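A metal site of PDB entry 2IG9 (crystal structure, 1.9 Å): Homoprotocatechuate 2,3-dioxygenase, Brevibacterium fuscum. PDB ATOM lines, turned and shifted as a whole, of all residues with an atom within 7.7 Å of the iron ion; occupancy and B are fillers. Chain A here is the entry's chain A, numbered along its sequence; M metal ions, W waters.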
ATOM      1  N   ASP A 154      -0.641 -19.363   7.207  1.00  0.00           N
ATOM      2  CA  ASP A 154       0.692 -19.407   6.569  1.00  0.00           C
ATOM      3  C   ASP A 154       1.637 -18.235   6.908  1.00  0.00           C
ATOM      4  O   ASP A 154       2.790 -18.475   7.238  1.00  0.00           O
ATOM      5  CB  ASP A 154       0.641 -19.622   5.039  1.00  0.00           C
ATOM      6  CG  ASP A 154       2.044 -19.953   4.487  1.00  0.00           C
ATOM      7  OD1 ASP A 154       2.512 -21.086   4.665  1.00  0.00           O
ATOM      8  OD2 ASP A 154       2.735 -19.051   3.962  1.00  0.00           O
ATOM      9  N   HIS A 155       1.148 -17.004   6.814  1.00  0.00           N
ATOM     10  CA  HIS A 155       2.011 -15.851   7.034  1.00  0.00           C
ATOM     11  C   HIS A 155       1.249 -14.555   7.150  1.00  0.00           C
ATOM     12  O   HIS A 155       0.042 -14.493   6.875  1.00  0.00           O
ATOM     13  CB  HIS A 155       3.018 -15.701   5.866  1.00  0.00           C
ATOM     14  CG  HIS A 155       2.366 -15.430   4.543  1.00  0.00           C
ATOM     15  ND1 HIS A 155       2.040 -16.437   3.663  1.00  0.00           N
ATOM     16  CD2 HIS A 155       1.953 -14.263   3.972  1.00  0.00           C
ATOM     17  CE1 HIS A 155       1.484 -15.904   2.583  1.00  0.00           C
ATOM     18  NE2 HIS A 155       1.423 -14.593   2.753  1.00  0.00           N
ATOM     19  N   PHE A 156       2.002 -13.509   7.524  1.00  0.00           N
ATOM     20  CA  PHE A 156       1.566 -12.115   7.505  1.00  0.00           C
ATOM     21  C   PHE A 156       2.319 -11.421   6.401  1.00  0.00           C
ATOM     22  O   PHE A 156       3.359 -11.932   5.950  1.00  0.00           O
ATOM     23  CB  PHE A 156       1.907 -11.447   8.828  1.00  0.00           C
ATOM     24  CG  PHE A 156       1.422 -12.217  10.044  1.00  0.00           C
ATOM     25  CD1 PHE A 156       0.055 -12.531  10.171  1.00  0.00           C
ATOM     26  CD2 PHE A 156       2.299 -12.660  11.009  1.00  0.00           C
ATOM     27  CE1 PHE A 156      -0.399 -13.219  11.276  1.00  0.00           C
ATOM     28  CE2 PHE A 156       1.831 -13.363  12.126  1.00  0.00           C
ATOM     29  CZ  PHE A 156       0.500 -13.655  12.249  1.00  0.00           C
ATOM     30  N   ASN A 157       1.788 -10.290   5.935  1.00  0.00           N
ATOM     31  CA  ASN A 157       2.521  -9.411   5.027  1.00  0.00           C
ATOM     32  C   ASN A 157       2.312  -7.975   5.536  1.00  0.00           C
ATOM     33  O   ASN A 157       1.164  -7.528   5.666  1.00  0.00           O
ATOM     34  CB  ASN A 157       2.031  -9.591   3.594  1.00  0.00           C
ATOM     35  CG  ASN A 157       2.939  -8.919   2.548  1.00  0.00           C
ATOM     36  OD1 ASN A 157       3.159  -7.703   2.586  1.00  0.00           O
ATOM     37  ND2 ASN A 157       3.470  -9.706   1.613  1.00  0.00           N
ATOM     38  N   TRP A 192      10.629 -11.421   1.353  1.00  0.00           N
ATOM     39  CA  TRP A 192       9.938 -12.505   2.061  1.00  0.00           C
ATOM     40  C   TRP A 192      10.916 -13.201   2.985  1.00  0.00           C
ATOM     41  O   TRP A 192      12.040 -13.451   2.574  1.00  0.00           O
ATOM     42  CB  TRP A 192       9.484 -13.543   1.032  1.00  0.00           C
ATOM     43  CG  TRP A 192       8.294 -13.102   0.204  1.00  0.00           C
ATOM     44  CD1 TRP A 192       7.029 -13.584   0.321  1.00  0.00           C
ATOM     45  CD2 TRP A 192       8.252 -12.094  -0.825  1.00  0.00           C
ATOM     46  NE1 TRP A 192       6.185 -12.947  -0.563  1.00  0.00           N
ATOM     47  CE2 TRP A 192       6.905 -12.027  -1.288  1.00  0.00           C
ATOM     48  CE3 TRP A 192       9.222 -11.248  -1.414  1.00  0.00           C
ATOM     49  CZ2 TRP A 192       6.489 -11.161  -2.322  1.00  0.00           C
ATOM     50  CZ3 TRP A 192       8.805 -10.373  -2.445  1.00  0.00           C
ATOM     51  CH2 TRP A 192       7.447 -10.343  -2.890  1.00  0.00           C
ATOM     52  N   HIS A 200       7.682 -18.038   3.617  1.00  0.00           N
ATOM     53  CA  HIS A 200       7.668 -16.941   4.588  1.00  0.00           C
ATOM     54  C   HIS A 200       6.728 -17.102   5.783  1.00  0.00           C
ATOM     55  O   HIS A 200       5.718 -17.823   5.696  1.00  0.00           O
ATOM     56  CB  HIS A 200       7.491 -15.578   3.934  1.00  0.00           C
ATOM     57  CG  HIS A 200       6.218 -15.396   3.150  1.00  0.00           C
ATOM     58  ND1 HIS A 200       5.713 -16.330   2.277  1.00  0.00           N
ATOM     59  CD2 HIS A 200       5.404 -14.318   3.050  1.00  0.00           C
ATOM     60  CE1 HIS A 200       4.637 -15.848   1.687  1.00  0.00           C
ATOM     61  NE2 HIS A 200       4.427 -14.625   2.135  1.00  0.00           N
ATOM     62  N   ALA A 203       6.291 -10.994   5.537  1.00  0.00           N
ATOM     63  CA  ALA A 203       6.935 -10.389   4.390  1.00  0.00           C
ATOM     64  C   ALA A 203       6.866  -8.875   4.527  1.00  0.00           C
ATOM     65  O   ALA A 203       6.042  -8.367   5.302  1.00  0.00           O
ATOM     66  CB  ALA A 203       6.261 -10.866   3.049  1.00  0.00           C
ATOM     67  N   THR A 205       6.400  -5.423   2.210  1.00  0.00           N
ATOM     68  CA  THR A 205       5.999  -4.848   0.978  1.00  0.00           C
ATOM     69  C   THR A 205       6.252  -3.354   1.128  1.00  0.00           C
ATOM     70  O   THR A 205       5.807  -2.752   2.101  1.00  0.00           O
ATOM     71  CB  THR A 205       4.505  -5.090   0.760  1.00  0.00           C
ATOM     72  OG1 THR A 205       4.236  -6.509   0.608  1.00  0.00           O
ATOM     73  CG2 THR A 205       3.990  -4.343  -0.443  1.00  0.00           C
ATOM     74  N   HIS A 213      -0.665  -5.540   5.258  1.00  0.00           N
ATOM     75  CA  HIS A 213      -1.137  -5.855   3.903  1.00  0.00           C
ATOM     76  C   HIS A 213      -2.171  -6.982   3.914  1.00  0.00           C
ATOM     77  O   HIS A 213      -3.308  -6.797   3.441  1.00  0.00           O
ATOM     78  CB  HIS A 213       0.007  -6.195   2.944  1.00  0.00           C
ATOM     79  CG  HIS A 213      -0.369  -5.998   1.521  1.00  0.00           C
ATOM     80  ND1 HIS A 213      -1.142  -6.896   0.824  1.00  0.00           N
ATOM     81  CD2 HIS A 213      -0.187  -4.947   0.687  1.00  0.00           C
ATOM     82  CE1 HIS A 213      -1.382  -6.436  -0.390  1.00  0.00           C
ATOM     83  NE2 HIS A 213      -0.822  -5.245  -0.502  1.00  0.00           N
ATOM     84  N   HIS A 214      -1.802  -8.131   4.466  1.00  0.00           N
ATOM     85  CA  HIS A 214      -2.737  -9.247   4.621  1.00  0.00           C
ATOM     86  C   HIS A 214      -2.264 -10.300   5.612  1.00  0.00           C
ATOM     87  O   HIS A 214      -1.115 -10.273   6.114  1.00  0.00           O
ATOM     88  CB  HIS A 214      -3.016  -9.940   3.275  1.00  0.00           C
ATOM     89  CG  HIS A 214      -1.796 -10.400   2.559  1.00  0.00           C
ATOM     90  ND1 HIS A 214      -1.086  -9.602   1.701  1.00  0.00           N
ATOM     91  CD2 HIS A 214      -1.127 -11.585   2.607  1.00  0.00           C
ATOM     92  CE1 HIS A 214      -0.051 -10.266   1.233  1.00  0.00           C
ATOM     93  NE2 HIS A 214      -0.052 -11.470   1.774  1.00  0.00           N
ATOM     94  N   VAL A 215      -3.199 -11.226   5.889  1.00  0.00           N
ATOM     95  CA  VAL A 215      -2.961 -12.447   6.618  1.00  0.00           C
ATOM     96  C   VAL A 215      -3.311 -13.539   5.618  1.00  0.00           C
ATOM     97  O   VAL A 215      -4.306 -13.447   4.894  1.00  0.00           O
ATOM     98  CB  VAL A 215      -3.935 -12.574   7.836  1.00  0.00           C
ATOM     99  CG1 VAL A 215      -3.800 -13.929   8.497  1.00  0.00           C
ATOM    100  CG2 VAL A 215      -3.704 -11.454   8.850  1.00  0.00           C
ATOM    101  N   ALA A 216      -2.497 -14.588   5.579  1.00  0.00           N
ATOM    102  CA  ALA A 216      -2.725 -15.629   4.608  1.00  0.00           C
ATOM    103  C   ALA A 216      -2.926 -16.983   5.251  1.00  0.00           C
ATOM    104  O   ALA A 216      -2.193 -17.387   6.200  1.00  0.00           O
ATOM    105  CB  ALA A 216      -1.572 -15.679   3.579  1.00  0.00           C
ATOM    106  N   HIS A 248       1.652 -17.340  -8.222  1.00  0.00           N
ATOM    107  CA  HIS A 248       2.707 -16.378  -7.834  1.00  0.00           C
ATOM    108  C   HIS A 248       4.034 -16.735  -8.517  1.00  0.00           C
ATOM    109  O   HIS A 248       4.376 -17.918  -8.699  1.00  0.00           O
ATOM    110  CB  HIS A 248       2.958 -16.418  -6.342  1.00  0.00           C
ATOM    111  CG  HIS A 248       2.006 -15.601  -5.503  1.00  0.00           C
ATOM    112  ND1 HIS A 248       1.619 -14.324  -5.848  1.00  0.00           N
ATOM    113  CD2 HIS A 248       1.393 -15.878  -4.323  1.00  0.00           C
ATOM    114  CE1 HIS A 248       0.803 -13.852  -4.913  1.00  0.00           C
ATOM    115  NE2 HIS A 248       0.657 -14.771  -3.976  1.00  0.00           N
ATOM    116  N   SER A 251       7.601 -17.178  -4.636  1.00  0.00           N
ATOM    117  CA  SER A 251       7.014 -18.244  -3.804  1.00  0.00           C
ATOM    118  C   SER A 251       6.357 -19.363  -4.600  1.00  0.00           C
ATOM    119  O   SER A 251       6.087 -20.398  -4.016  1.00  0.00           O
ATOM    120  CB  SER A 251       6.001 -17.708  -2.773  1.00  0.00           C
ATOM    121  OG  SER A 251       4.683 -17.666  -3.316  1.00  0.00           O
ATOM    122  N   TYR A 255      -2.713 -18.727  -5.527  1.00  0.00           N
ATOM    123  CA  TYR A 255      -3.102 -17.656  -4.617  1.00  0.00           C
ATOM    124  C   TYR A 255      -4.451 -17.019  -4.980  1.00  0.00           C
ATOM    125  O   TYR A 255      -4.942 -17.135  -6.119  1.00  0.00           O
ATOM    126  CB  TYR A 255      -1.984 -16.585  -4.506  1.00  0.00           C
ATOM    127  CG  TYR A 255      -1.950 -15.652  -5.714  1.00  0.00           C
ATOM    128  CD1 TYR A 255      -1.089 -15.894  -6.789  1.00  0.00           C
ATOM    129  CD2 TYR A 255      -2.842 -14.564  -5.811  1.00  0.00           C
ATOM    130  CE1 TYR A 255      -1.088 -15.052  -7.921  1.00  0.00           C
ATOM    131  CE2 TYR A 255      -2.847 -13.725  -6.935  1.00  0.00           C
ATOM    132  CZ  TYR A 255      -1.984 -13.976  -7.984  1.00  0.00           C
ATOM    133  OH  TYR A 255      -1.979 -13.158  -9.079  1.00  0.00           O
ATOM    134  N   LEU A 256      -5.015 -16.332  -3.971  1.00  0.00           N
ATOM    135  CA  LEU A 256      -6.212 -15.526  -4.130  1.00  0.00           C
ATOM    136  C   LEU A 256      -6.202 -14.448  -3.048  1.00  0.00           C
ATOM    137  O   LEU A 256      -5.783 -14.737  -1.934  1.00  0.00           O
ATOM    138  CB  LEU A 256      -7.461 -16.390  -3.927  1.00  0.00           C
ATOM    139  CG  LEU A 256      -8.778 -15.636  -3.933  1.00  0.00           C
ATOM    140  CD1 LEU A 256      -9.067 -15.133  -5.353  1.00  0.00           C
ATOM    141  CD2 LEU A 256      -9.844 -16.576  -3.406  1.00  0.00           C
ATOM    142  N   TYR A 257      -6.657 -13.239  -3.381  1.00  0.00           N
ATOM    143  CA  TYR A 257      -6.862 -12.158  -2.388  1.00  0.00           C
ATOM    144  C   TYR A 257      -8.299 -11.713  -2.388  1.00  0.00           C
ATOM    145  O   TYR A 257      -8.883 -11.414  -3.436  1.00  0.00           O
ATOM    146  CB  TYR A 257      -5.983 -10.914  -2.658  1.00  0.00           C
ATOM    147  CG  TYR A 257      -4.507 -11.214  -2.738  1.00  0.00           C
ATOM    148  CD1 TYR A 257      -3.747 -11.260  -1.573  1.00  0.00           C
ATOM    149  CD2 TYR A 257      -3.887 -11.474  -3.961  1.00  0.00           C
ATOM    150  CE1 TYR A 257      -2.386 -11.546  -1.598  1.00  0.00           C
ATOM    151  CE2 TYR A 257      -2.506 -11.766  -3.999  1.00  0.00           C
ATOM    152  CZ  TYR A 257      -1.774 -11.784  -2.820  1.00  0.00           C
ATOM    153  OH  TYR A 257      -0.435 -12.049  -2.844  1.00  0.00           O
ATOM    154  N   GLU A 267      -5.405 -13.435   2.121  1.00  0.00           N
ATOM    155  CA  GLU A 267      -4.884 -14.256   1.015  1.00  0.00           C
ATOM    156  C   GLU A 267      -5.115 -15.732   1.315  1.00  0.00           C
ATOM    157  O   GLU A 267      -5.032 -16.150   2.447  1.00  0.00           O
ATOM    158  CB  GLU A 267      -3.389 -14.026   0.791  1.00  0.00           C
ATOM    159  CG  GLU A 267      -2.837 -14.827  -0.431  1.00  0.00           C
ATOM    160  CD  GLU A 267      -1.319 -14.678  -0.580  1.00  0.00           C
ATOM    161  OE1 GLU A 267      -0.726 -14.065   0.327  1.00  0.00           O
ATOM    162  OE2 GLU A 267      -0.741 -15.135  -1.606  1.00  0.00           O
ATOM    163  N   ILE A 268      -5.414 -16.485   0.259  1.00  0.00           N
ATOM    164  CA  ILE A 268      -5.534 -17.950   0.318  1.00  0.00           C
ATOM    165  C   ILE A 268      -4.417 -18.435  -0.592  1.00  0.00           C
ATOM    166  O   ILE A 268      -4.190 -17.820  -1.633  1.00  0.00           O
ATOM    167  CB  ILE A 268      -6.927 -18.478  -0.173  1.00  0.00           C
ATOM    168  CG1 ILE A 268      -8.078 -17.621   0.384  1.00  0.00           C
ATOM    169  CG2 ILE A 268      -7.081 -19.947   0.197  1.00  0.00           C
ATOM    170  CD1 ILE A 268      -8.131 -17.533   1.916  1.00  0.00           C
ATOM    171  N   TYR A 269      -3.723 -19.487  -0.175  1.00  0.00           N
ATOM    172  CA  TYR A 269      -2.351 -19.786  -0.607  1.00  0.00           C
ATOM    173  C   TYR A 269      -2.111 -21.291  -0.510  1.00  0.00           C
ATOM    174  O   TYR A 269      -2.524 -21.925   0.445  1.00  0.00           O
ATOM    175  CB  TYR A 269      -1.440 -19.050   0.387  1.00  0.00           C
ATOM    176  CG  TYR A 269       0.043 -19.059   0.207  1.00  0.00           C
ATOM    177  CD1 TYR A 269       0.702 -18.020  -0.462  1.00  0.00           C
ATOM    178  CD2 TYR A 269       0.830 -20.065   0.789  1.00  0.00           C
ATOM    179  CE1 TYR A 269       2.100 -18.005  -0.556  1.00  0.00           C
ATOM    180  CE2 TYR A 269       2.192 -20.067   0.685  1.00  0.00           C
ATOM    181  CZ  TYR A 269       2.830 -19.036   0.008  1.00  0.00           C
ATOM    182  OH  TYR A 269       4.209 -19.052  -0.058  1.00  0.00           O
ATOM    183  N   ARG A 293       4.894 -11.459  -9.869  1.00  0.00           N
ATOM    184  CA  ARG A 293       3.802 -11.438  -8.879  1.00  0.00           C
ATOM    185  C   ARG A 293       2.729 -12.433  -9.322  1.00  0.00           C
ATOM    186  O   ARG A 293       2.323 -13.295  -8.564  1.00  0.00           O
ATOM    187  CB  ARG A 293       3.276 -10.014  -8.651  1.00  0.00           C
ATOM    188  CG  ARG A 293       4.235  -9.166  -7.796  1.00  0.00           C
ATOM    189  CD  ARG A 293       3.578  -7.943  -7.121  1.00  0.00           C
ATOM    190  NE  ARG A 293       4.500  -7.209  -6.242  1.00  0.00           N
ATOM    191  CZ  ARG A 293       4.771  -7.527  -4.980  1.00  0.00           C
ATOM    192  NH1 ARG A 293       4.182  -8.562  -4.385  1.00  0.00           N
ATOM    193  NH2 ARG A 293       5.639  -6.800  -4.287  1.00  0.00           N
ATOM    194  N   TRP A 304      -4.249  -3.352  -4.758  1.00  0.00           N
ATOM    195  CA  TRP A 304      -3.278  -4.220  -4.092  1.00  0.00           C
ATOM    196  C   TRP A 304      -2.029  -3.462  -3.646  1.00  0.00           C
ATOM    197  O   TRP A 304      -1.446  -3.761  -2.599  1.00  0.00           O
ATOM    198  CB  TRP A 304      -2.909  -5.412  -5.020  1.00  0.00           C
ATOM    199  CG  TRP A 304      -2.436  -6.578  -4.274  1.00  0.00           C
ATOM    200  CD1 TRP A 304      -3.178  -7.620  -3.802  1.00  0.00           C
ATOM    201  CD2 TRP A 304      -1.092  -6.825  -3.875  1.00  0.00           C
ATOM    202  NE1 TRP A 304      -2.371  -8.508  -3.133  1.00  0.00           N
ATOM    203  CE2 TRP A 304      -1.077  -8.043  -3.176  1.00  0.00           C
ATOM    204  CE3 TRP A 304       0.112  -6.139  -4.055  1.00  0.00           C
ATOM    205  CZ2 TRP A 304       0.080  -8.579  -2.643  1.00  0.00           C
ATOM    206  CZ3 TRP A 304       1.254  -6.670  -3.535  1.00  0.00           C
ATOM    207  CH2 TRP A 304       1.228  -7.885  -2.815  1.00  0.00           C
HETATM  208 FE    FE M   1       1.080 -13.225   0.819  1.00  0.00          FE
HETATM  209  O   HOH W   1       2.077 -14.785  -0.526  1.00  0.00           O
HETATM  210  O   HOH W   2       1.330 -12.020  -1.038  1.00  0.00           O
HETATM  211  O   HOH W   3       3.015 -12.439   1.309  1.00  0.00           O
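The iron ion is bound by the side-chain carboxylate (OE1) of Glu 267, at 2.1 Å. The iron ion is bound by water W3 (2.1 Å). Water W2 binds the iron ion, at 2.2 Å. The iron ion is bound by water W1 (2.3 Å). NE2 of His 214 is bound to the iron ion (2.3 Å). The iron ion is bound by NE2 of His 155 (2.4 Å). The iron ion has six donor atoms within binding distance.
The side-chain carboxylate (OE2) of Glu 267 is in hydrogen-bond range of the side-chain hydroxyl (OH) of Tyr 257, 3.3 Å away. A ring nitrogen (NE2) of His 248 is in hydrogen-bond range of the side-chain carboxylate (OE2) of Glu 267, at 2.8 Å. O of Val 215 lies within hydrogen-bond range of N of Glu 267 (3.0 Å). The backbone carbonyl oxygen (O) of His 214 sits at hydrogen-bond distance from the backbone NH (N) of Asn 157 (2.9 Å). A ring nitrogen (ND1) of His 213 sits at hydrogen-bond distance from a ring nitrogen (ND1) of His 214, at 2.8 Å. A ring nitrogen (ND1) of His 155 sits close to a ring nitrogen (NE2) of His 200 (3.4 Å). The backbone NH of Ala 216 is in hydrogen-bond range of the backbone carbonyl oxygen of His 155 (2.9 Å). OD2 of Asp 154 sits at hydrogen-bond distance from ND1 of His 155 (2.7 Å).
NE2 of His 200 touches the iron ion, 3.9 Å away.
Water W3 bridges NE2 of His 200 and ND2 of Asn 157.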
